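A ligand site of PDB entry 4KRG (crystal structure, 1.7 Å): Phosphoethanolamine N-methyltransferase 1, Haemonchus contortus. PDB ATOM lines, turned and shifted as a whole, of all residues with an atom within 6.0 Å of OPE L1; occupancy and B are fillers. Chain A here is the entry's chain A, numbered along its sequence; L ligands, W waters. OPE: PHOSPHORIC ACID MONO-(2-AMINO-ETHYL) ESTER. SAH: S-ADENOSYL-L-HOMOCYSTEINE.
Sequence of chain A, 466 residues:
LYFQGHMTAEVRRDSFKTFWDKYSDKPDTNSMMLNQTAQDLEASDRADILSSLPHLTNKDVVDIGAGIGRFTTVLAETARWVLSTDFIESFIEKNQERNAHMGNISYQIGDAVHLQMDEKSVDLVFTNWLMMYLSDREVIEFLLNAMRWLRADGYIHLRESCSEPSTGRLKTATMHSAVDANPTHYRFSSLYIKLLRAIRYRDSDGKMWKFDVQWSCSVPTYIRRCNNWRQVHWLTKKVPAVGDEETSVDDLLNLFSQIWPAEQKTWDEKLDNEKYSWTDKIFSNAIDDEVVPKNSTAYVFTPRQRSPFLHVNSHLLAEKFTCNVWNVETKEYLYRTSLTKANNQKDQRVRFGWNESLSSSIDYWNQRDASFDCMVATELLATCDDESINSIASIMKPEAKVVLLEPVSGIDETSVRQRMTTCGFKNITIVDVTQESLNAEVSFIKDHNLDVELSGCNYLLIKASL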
ATOM      1  N   TRP A  20      31.976 -21.150  20.226  1.00  0.00           N
ATOM      2  CA  TRP A  20      32.221 -20.062  19.290  1.00  0.00           C
ATOM      3  C   TRP A  20      33.513 -20.237  18.507  1.00  0.00           C
ATOM      4  O   TRP A  20      33.645 -19.709  17.407  1.00  0.00           O
ATOM      5  CB  TRP A  20      32.126 -18.704  19.990  1.00  0.00           C
ATOM      6  CG  TRP A  20      30.700 -18.265  20.107  1.00  0.00           C
ATOM      7  CD1 TRP A  20      29.936 -18.243  21.227  1.00  0.00           C
ATOM      8  CD2 TRP A  20      29.874 -17.841  19.029  1.00  0.00           C
ATOM      9  NE1 TRP A  20      28.670 -17.811  20.918  1.00  0.00           N
ATOM     10  CE2 TRP A  20      28.595 -17.556  19.571  1.00  0.00           C
ATOM     11  CE3 TRP A  20      30.064 -17.663  17.658  1.00  0.00           C
ATOM     12  CZ2 TRP A  20      27.546 -17.108  18.786  1.00  0.00           C
ATOM     13  CZ3 TRP A  20      29.020 -17.221  16.885  1.00  0.00           C
ATOM     14  CH2 TRP A  20      27.766 -16.947  17.445  1.00  0.00           C
ATOM     15  N   SER A  31      27.645 -16.466  10.862  1.00  0.00           N
ATOM     16  CA  SER A  31      28.005 -16.888  12.213  1.00  0.00           C
ATOM     17  C   SER A  31      27.376 -16.020  13.297  1.00  0.00           C
ATOM     18  O   SER A  31      26.896 -16.520  14.322  1.00  0.00           O
ATOM     19  CB  SER A  31      29.525 -16.899  12.386  1.00  0.00           C
ATOM     20  OG  SER A  31      30.086 -18.007  11.702  1.00  0.00           O
ATOM     21  N   MET A  32      27.379 -14.703  13.058  1.00  0.00           N
ATOM     22  CA  MET A  32      26.845 -13.730  14.007  1.00  0.00           C
ATOM     23  C   MET A  32      25.395 -13.997  14.296  1.00  0.00           C
ATOM     24  O   MET A  32      24.910 -13.766  15.399  1.00  0.00           O
ATOM     25  CB  MET A  32      26.987 -12.315  13.437  1.00  0.00           C
ATOM     26  CG  MET A  32      28.418 -11.894  13.133  1.00  0.00           C
ATOM     27  SD  MET A  32      29.605 -12.062  14.689  1.00  0.00           S
ATOM     28  CE  MET A  32      30.291 -13.853  14.359  1.00  0.00           C
ATOM     29  N   MET A  33      24.685 -14.475  13.286  1.00  0.00           N
ATOM     30  CA  MET A  33      23.251 -14.685  13.416  1.00  0.00           C
ATOM     31  C   MET A  33      22.932 -16.167  13.468  1.00  0.00           C
ATOM     32  O   MET A  33      21.781 -16.538  13.694  1.00  0.00           O
ATOM     33  CB  MET A  33      22.528 -14.006  12.258  1.00  0.00           C
ATOM     34  CG  MET A  33      22.957 -12.554  12.072  1.00  0.00           C
ATOM     35  SD  MET A  33      21.889 -11.621  10.726  1.00  0.00           S
ATOM     36  CE  MET A  33      20.425 -10.985  11.861  1.00  0.00           C
ATOM     37  N   LEU A  34      23.964 -17.002  13.310  1.00  0.00           N
ATOM     38  CA  LEU A  34      23.800 -18.467  13.265  1.00  0.00           C
ATOM     39  C   LEU A  34      22.695 -18.873  12.298  1.00  0.00           C
ATOM     40  O   LEU A  34      21.783 -19.625  12.638  1.00  0.00           O
ATOM     41  CB  LEU A  34      23.584 -19.047  14.673  1.00  0.00           C
ATOM     42  CG  LEU A  34      24.827 -18.921  15.558  1.00  0.00           C
ATOM     43  CD1 LEU A  34      24.568 -19.408  16.973  1.00  0.00           C
ATOM     44  CD2 LEU A  34      25.994 -19.681  14.946  1.00  0.00           C
ATOM     45  N   TRP A 129      22.343 -10.447  21.608  1.00  0.00           N
ATOM     46  CA  TRP A 129      22.632 -11.883  21.731  1.00  0.00           C
ATOM     47  C   TRP A 129      23.841 -12.204  22.635  1.00  0.00           C
ATOM     48  O   TRP A 129      24.847 -12.707  22.144  1.00  0.00           O
ATOM     49  CB  TRP A 129      22.873 -12.527  20.348  1.00  0.00           C
ATOM     50  CG  TRP A 129      21.677 -12.695  19.460  1.00  0.00           C
ATOM     51  CD1 TRP A 129      20.424 -13.122  19.812  1.00  0.00           C
ATOM     52  CD2 TRP A 129      21.647 -12.461  18.055  1.00  0.00           C
ATOM     53  NE1 TRP A 129      19.616 -13.173  18.699  1.00  0.00           N
ATOM     54  CE2 TRP A 129      20.338 -12.778  17.606  1.00  0.00           C
ATOM     55  CE3 TRP A 129      22.592 -12.029  17.109  1.00  0.00           C
ATOM     56  CZ2 TRP A 129      19.969 -12.662  16.262  1.00  0.00           C
ATOM     57  CZ3 TRP A 129      22.216 -11.923  15.796  1.00  0.00           C
ATOM     58  CH2 TRP A 129      20.913 -12.234  15.380  1.00  0.00           C
ATOM     59  N   MET A 132      22.287 -14.997  26.772  1.00  0.00           N
ATOM     60  CA  MET A 132      21.995 -16.398  26.476  1.00  0.00           C
ATOM     61  C   MET A 132      23.270 -17.253  26.458  1.00  0.00           C
ATOM     62  O   MET A 132      23.192 -18.478  26.487  1.00  0.00           O
ATOM     63  CB  MET A 132      21.294 -16.495  25.126  1.00  0.00           C
ATOM     64  CG  MET A 132      22.116 -15.863  24.027  1.00  0.00           C
ATOM     65  SD  MET A 132      21.087 -15.309  22.461  1.00  0.00           S
ATOM     66  CE  MET A 132      20.917 -17.060  21.587  1.00  0.00           C
ATOM     67  N   TYR A 133      24.431 -16.595  26.394  1.00  0.00           N
ATOM     68  CA  TYR A 133      25.714 -17.300  26.431  1.00  0.00           C
ATOM     69  C   TYR A 133      26.418 -17.153  27.786  1.00  0.00           C
ATOM     70  O   TYR A 133      27.607 -17.440  27.909  1.00  0.00           O
ATOM     71  CB  TYR A 133      26.632 -16.822  25.296  1.00  0.00           C
ATOM     72  CG  TYR A 133      26.033 -16.994  23.909  1.00  0.00           C
ATOM     73  CD1 TYR A 133      25.749 -18.259  23.409  1.00  0.00           C
ATOM     74  CD2 TYR A 133      25.751 -15.887  23.112  1.00  0.00           C
ATOM     75  CE1 TYR A 133      25.204 -18.413  22.149  1.00  0.00           C
ATOM     76  CE2 TYR A 133      25.199 -16.034  21.849  1.00  0.00           C
ATOM     77  CZ  TYR A 133      24.924 -17.310  21.375  1.00  0.00           C
ATOM     78  OH  TYR A 133      24.370 -17.469  20.123  1.00  0.00           O
ATOM     79  N   SER A 161      17.583 -14.320  22.394  1.00  0.00           N
ATOM     80  CA  SER A 161      16.704 -15.365  21.895  1.00  0.00           C
ATOM     81  C   SER A 161      15.998 -15.937  23.100  1.00  0.00           C
ATOM     82  O   SER A 161      16.627 -16.590  23.938  1.00  0.00           O
ATOM     83  CB  SER A 161      17.489 -16.458  21.186  1.00  0.00           C
ATOM     84  OG  SER A 161      18.182 -15.939  20.068  1.00  0.00           O
ATOM     85  N   GLU A 164      13.524 -20.174  22.714  1.00  0.00           N
ATOM     86  CA  GLU A 164      13.910 -21.035  21.607  1.00  0.00           C
ATOM     87  C   GLU A 164      14.944 -20.335  20.722  1.00  0.00           C
ATOM     88  O   GLU A 164      15.091 -19.117  20.795  1.00  0.00           O
ATOM     89  CB  GLU A 164      12.691 -21.377  20.757  1.00  0.00           C
ATOM     90  CG  GLU A 164      12.216 -20.233  19.884  1.00  0.00           C
ATOM     91  CD  GLU A 164      10.927 -20.538  19.157  1.00  0.00           C
ATOM     92  OE1 GLU A 164      10.961 -20.639  17.907  1.00  0.00           O
ATOM     93  OE2 GLU A 164       9.879 -20.669  19.816  1.00  0.00           O
ATOM     94  N   PRO A 165      15.664 -21.097  19.888  1.00  0.00           N
ATOM     95  CA  PRO A 165      16.647 -20.408  19.032  1.00  0.00           C
ATOM     96  C   PRO A 165      15.965 -19.461  18.058  1.00  0.00           C
ATOM     97  O   PRO A 165      14.784 -19.636  17.738  1.00  0.00           O
ATOM     98  CB  PRO A 165      17.310 -21.561  18.267  1.00  0.00           C
ATOM     99  CG  PRO A 165      17.072 -22.768  19.117  1.00  0.00           C
ATOM    100  CD  PRO A 165      15.705 -22.557  19.698  1.00  0.00           C
ATOM    101  N   SER A 166      16.711 -18.473  17.580  1.00  0.00           N
ATOM    102  CA  SER A 166      16.190 -17.498  16.633  1.00  0.00           C
ATOM    103  C   SER A 166      15.526 -18.191  15.456  1.00  0.00           C
ATOM    104  O   SER A 166      14.483 -17.753  14.966  1.00  0.00           O
ATOM    105  CB  SER A 166      17.298 -16.595  16.127  1.00  0.00           C
ATOM    106  OG  SER A 166      18.235 -17.331  15.357  1.00  0.00           O
ATOM    107  N   THR A 167      16.142 -19.280  15.004  1.00  0.00           N
ATOM    108  CA  THR A 167      15.651 -20.056  13.883  1.00  0.00           C
ATOM    109  C   THR A 167      14.679 -21.169  14.297  1.00  0.00           C
ATOM    110  O   THR A 167      14.467 -22.118  13.545  1.00  0.00           O
ATOM    111  CB  THR A 167      16.813 -20.666  13.062  1.00  0.00           C
ATOM    112  OG1 THR A 167      17.694 -21.366  13.952  1.00  0.00           O
ATOM    113  CG2 THR A 167      17.575 -19.585  12.336  1.00  0.00           C
ATOM    114  N   THR A 174      19.164 -22.897  10.467  1.00  0.00           N
ATOM    115  CA  THR A 174      20.160 -22.822  11.523  1.00  0.00           C
ATOM    116  C   THR A 174      21.572 -23.198  11.081  1.00  0.00           C
ATOM    117  O   THR A 174      21.774 -24.007  10.168  1.00  0.00           O
ATOM    118  CB  THR A 174      19.765 -23.666  12.742  1.00  0.00           C
ATOM    119  OG1 THR A 174      20.501 -23.226  13.889  1.00  0.00           O
ATOM    120  CG2 THR A 174      20.042 -25.146  12.492  1.00  0.00           C
ATOM    121  N   HIS A 176      23.454 -24.072  13.655  1.00  0.00           N
ATOM    122  CA  HIS A 176      23.703 -24.989  14.741  1.00  0.00           C
ATOM    123  C   HIS A 176      23.950 -26.383  14.190  1.00  0.00           C
ATOM    124  O   HIS A 176      23.503 -26.726  13.096  1.00  0.00           O
ATOM    125  CB  HIS A 176      22.527 -25.023  15.708  1.00  0.00           C
ATOM    126  CG  HIS A 176      22.484 -23.859  16.645  1.00  0.00           C
ATOM    127  ND1 HIS A 176      23.418 -23.680  17.640  1.00  0.00           N
ATOM    128  CD2 HIS A 176      21.619 -22.817  16.736  1.00  0.00           C
ATOM    129  CE1 HIS A 176      23.134 -22.578  18.303  1.00  0.00           C
ATOM    130  NE2 HIS A 176      22.050 -22.031  17.777  1.00  0.00           N
ATOM    131  N   ASN A 182      23.321 -28.114  22.089  1.00  0.00           N
ATOM    132  CA  ASN A 182      23.405 -26.659  22.020  1.00  0.00           C
ATOM    133  C   ASN A 182      23.414 -26.099  23.439  1.00  0.00           C
ATOM    134  O   ASN A 182      22.425 -26.221  24.154  1.00  0.00           O
ATOM    135  CB  ASN A 182      22.218 -26.123  21.218  1.00  0.00           C
ATOM    136  CG  ASN A 182      22.300 -24.634  20.977  1.00  0.00           C
ATOM    137  OD1 ASN A 182      23.289 -23.983  21.297  1.00  0.00           O
ATOM    138  ND2 ASN A 182      21.236 -24.086  20.404  1.00  0.00           N
ATOM    139  N   THR A 184      23.447 -23.090  24.545  1.00  0.00           N
ATOM    140  CA  THR A 184      22.772 -21.807  24.706  1.00  0.00           C
ATOM    141  C   THR A 184      21.650 -21.843  25.750  1.00  0.00           C
ATOM    142  O   THR A 184      20.912 -22.825  25.853  1.00  0.00           O
ATOM    143  CB  THR A 184      22.231 -21.329  23.362  1.00  0.00           C
ATOM    144  OG1 THR A 184      23.247 -21.459  22.365  1.00  0.00           O
ATOM    145  CG2 THR A 184      21.768 -19.891  23.433  1.00  0.00           C
ATOM    146  N   TYR A 186      18.245 -20.500  26.475  1.00  0.00           N
ATOM    147  CA  TYR A 186      17.069 -19.823  25.917  1.00  0.00           C
ATOM    148  C   TYR A 186      16.055 -19.585  27.026  1.00  0.00           C
ATOM    149  O   TYR A 186      15.190 -20.411  27.284  1.00  0.00           O
ATOM    150  CB  TYR A 186      16.459 -20.652  24.783  1.00  0.00           C
ATOM    151  CG  TYR A 186      17.438 -20.899  23.667  1.00  0.00           C
ATOM    152  CD1 TYR A 186      17.796 -19.894  22.792  1.00  0.00           C
ATOM    153  CD2 TYR A 186      18.022 -22.151  23.488  1.00  0.00           C
ATOM    154  CE1 TYR A 186      18.699 -20.109  21.766  1.00  0.00           C
ATOM    155  CE2 TYR A 186      18.923 -22.392  22.475  1.00  0.00           C
ATOM    156  CZ  TYR A 186      19.252 -21.363  21.621  1.00  0.00           C
ATOM    157  OH  TYR A 186      20.146 -21.583  20.604  1.00  0.00           O
ATOM    158  N   TYR A 222      12.440 -10.617  12.624  1.00  0.00           N
ATOM    159  CA  TYR A 222      12.275 -12.017  12.998  1.00  0.00           C
ATOM    160  C   TYR A 222      10.819 -12.465  13.007  1.00  0.00           C
ATOM    161  O   TYR A 222      10.535 -13.646  12.861  1.00  0.00           O
ATOM    162  CB  TYR A 222      13.009 -12.341  14.299  1.00  0.00           C
ATOM    163  CG  TYR A 222      14.438 -12.695  14.014  1.00  0.00           C
ATOM    164  CD1 TYR A 222      14.811 -14.020  13.790  1.00  0.00           C
ATOM    165  CD2 TYR A 222      15.413 -11.712  13.899  1.00  0.00           C
ATOM    166  CE1 TYR A 222      16.108 -14.348  13.498  1.00  0.00           C
ATOM    167  CE2 TYR A 222      16.724 -12.039  13.612  1.00  0.00           C
ATOM    168  CZ  TYR A 222      17.068 -13.368  13.412  1.00  0.00           C
ATOM    169  OH  TYR A 222      18.366 -13.711  13.122  1.00  0.00           O
ATOM    170  N   GLN A 231      12.319 -13.205  19.593  1.00  0.00           N
ATOM    171  CA  GLN A 231      13.539 -12.414  19.559  1.00  0.00           C
ATOM    172  C   GLN A 231      13.200 -11.116  20.254  1.00  0.00           C
ATOM    173  O   GLN A 231      12.624 -10.209  19.647  1.00  0.00           O
ATOM    174  CB  GLN A 231      13.961 -12.156  18.123  1.00  0.00           C
ATOM    175  CG  GLN A 231      14.439 -13.403  17.416  1.00  0.00           C
ATOM    176  CD  GLN A 231      15.725 -13.911  18.000  1.00  0.00           C
ATOM    177  OE1 GLN A 231      16.758 -13.254  17.893  1.00  0.00           O
ATOM    178  NE2 GLN A 231      15.676 -15.079  18.645  1.00  0.00           N
HETATM  179  CA  OPE L   1      21.407 -16.504  17.188  1.00  0.00           C
HETATM  180  CB  OPE L   1      22.721 -15.854  16.896  1.00  0.00           C
HETATM  181  O1  OPE L   1      19.866 -18.904  16.823  1.00  0.00           O
HETATM  182  O2  OPE L   1      19.123 -17.890  18.920  1.00  0.00           O
HETATM  183  O3  OPE L   1      20.760 -19.768  19.000  1.00  0.00           O
HETATM  184  O4  OPE L   1      21.449 -17.516  18.128  1.00  0.00           O
HETATM  185  N   OPE L   1      23.501 -15.396  18.010  1.00  0.00           N
HETATM  186  P   OPE L   1      20.283 -18.553  18.231  1.00  0.00           P
HETATM  187  N   SAH L   2      26.407  -9.172  18.890  1.00  0.00           N
HETATM  188  CA  SAH L   2      26.867  -9.502  17.533  1.00  0.00           C
HETATM  189  CB  SAH L   2      27.294 -11.007  17.504  1.00  0.00           C
HETATM  190  CG  SAH L   2      26.210 -11.970  17.983  1.00  0.00           C
HETATM  191  SD  SAH L   2      26.733 -13.698  18.186  1.00  0.00           S
HETATM  192  C   SAH L   2      25.817  -9.221  16.530  1.00  0.00           C
HETATM  193  O   SAH L   2      24.648  -9.377  16.816  1.00  0.00           O
HETATM  194  OXT SAH L   2      26.143  -9.148  15.365  1.00  0.00           O
HETATM  195  C5' SAH L   2      27.612 -13.736  19.779  1.00  0.00           C
HETATM  196  C4' SAH L   2      28.824 -12.999  19.927  1.00  0.00           C
HETATM  197  O4' SAH L   2      29.101 -12.793  21.339  1.00  0.00           O
HETATM  198  C3' SAH L   2      29.980 -13.729  19.381  1.00  0.00           C
HETATM  199  O3' SAH L   2      30.868 -12.816  18.763  1.00  0.00           O
HETATM  200  C2' SAH L   2      30.623 -14.308  20.546  1.00  0.00           C
HETATM  201  O2' SAH L   2      31.990 -14.504  20.329  1.00  0.00           O
HETATM  202  C1' SAH L   2      30.369 -13.289  21.594  1.00  0.00           C
HETATM  203  N9  SAH L   2      30.450 -13.829  23.002  1.00  0.00           N
HETATM  204  C8  SAH L   2      29.707 -14.799  23.551  1.00  0.00           C
HETATM  205  N7  SAH L   2      30.018 -14.843  24.849  1.00  0.00           N
HETATM  206  C5  SAH L   2      30.939 -13.921  25.125  1.00  0.00           C
HETATM  207  C6  SAH L   2      31.613 -13.536  26.294  1.00  0.00           C
HETATM  208  N6  SAH L   2      31.373 -14.166  27.494  1.00  0.00           N
HETATM  209  N1  SAH L   2      32.504 -12.534  26.217  1.00  0.00           N
HETATM  210  C2  SAH L   2      32.753 -11.903  25.072  1.00  0.00           C
HETATM  211  N3  SAH L   2      32.121 -12.249  23.930  1.00  0.00           N
HETATM  212  C4  SAH L   2      31.220 -13.247  23.930  1.00  0.00           C
HETATM  213  O   HOH W   1      23.240 -19.860  19.833  1.00  0.00           O
HETATM  214  O   HOH W   2      20.056 -20.626  14.517  1.00  0.00           O
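The side-chain sulfur (SD) of Met 132 lies within hydrogen-bond range of the backbone NH (N) of Ser 161 (3.6 Å).
The indole nitrogen (NE1) of Trp 129 sits at hydrogen-bond distance from the side-chain amide oxygen (OE1) of Gln 231 (3.0 Å).
A ring nitrogen (NE2) of His 176 lies close to the side-chain amide nitrogen (ND2) of Asn 182.
NE2 of Gln 231 is in hydrogen-bond range of OG of Ser 161, 3.0 Å away.
The side-chain hydroxyl (OH) of Tyr 186 lies within hydrogen-bond range of the side-chain amide nitrogen (ND2) of Asn 182 (2.7 Å).
The indole nitrogen (NE1) of Trp 129 sits at hydrogen-bond distance from the side-chain hydroxyl (OG) of Ser 161, at 3.4 Å.
The backbone NH of His 176 sits at hydrogen-bond distance from the side-chain hydroxyl of Thr 174.
OH of Tyr 186 is in hydrogen-bond range of NE2 of His 176 (3.4 Å).
Water W1 lies within hydrogen-bond range of an oxygen (O3) of OPE L1 (2.6 Å), the side-chain hydroxyl (OH) of Tyr 133 (2.7 Å), the side-chain hydroxyl (OG1) of Thr 184 (3.0 Å) and a ring nitrogen (NE2) of His 176 (3.2 Å).
Water W2 lies within hydrogen-bond range of the side-chain hydroxyl of Thr 167 (2.5 Å), the side-chain hydroxyl of Thr 174 (2.7 Å), the backbone carbonyl oxygen of Leu 34 (2.7 Å) and an oxygen (O1) of OPE L1 (2.9 Å).
Residues that only touch OPE L1: Met 132 (3.3 Å), Met 33 (3.4 Å), Trp 129 (3.5 Å), Pro 165 (3.5 Å) and Leu 34 (3.8 Å).
The nearest printed residue that does not touch OPE L1 is Thr 167 (4.2 Å).
A nitrogen (N) of OPE L1 sits close to a sulfur (SD) of SAH L2.
An oxygen (O3) of OPE L1 lies within hydrogen-bond range of a ring nitrogen (NE2) of His 176, 2.9 Å away.
The backbone NH (N) of Ser 166 sits at hydrogen-bond distance from an oxygen (O2) of OPE L1, at 2.8 Å.
OH of Tyr 133 sits at hydrogen-bond distance from N of OPE L1, 3.1 Å away.
O3 of OPE L1 is in hydrogen-bond range of OH of Tyr 186.
The side-chain hydroxyl (OG) of Ser 161 sits at hydrogen-bond distance from an oxygen (O2) of OPE L1 (2.5 Å).
The side-chain hydroxyl of Ser 166 is in hydrogen-bond range of an oxygen (O1) of OPE L1 (2.7 Å).
O of Met 32 sits close to N of OPE L1, 3.4 Å away.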
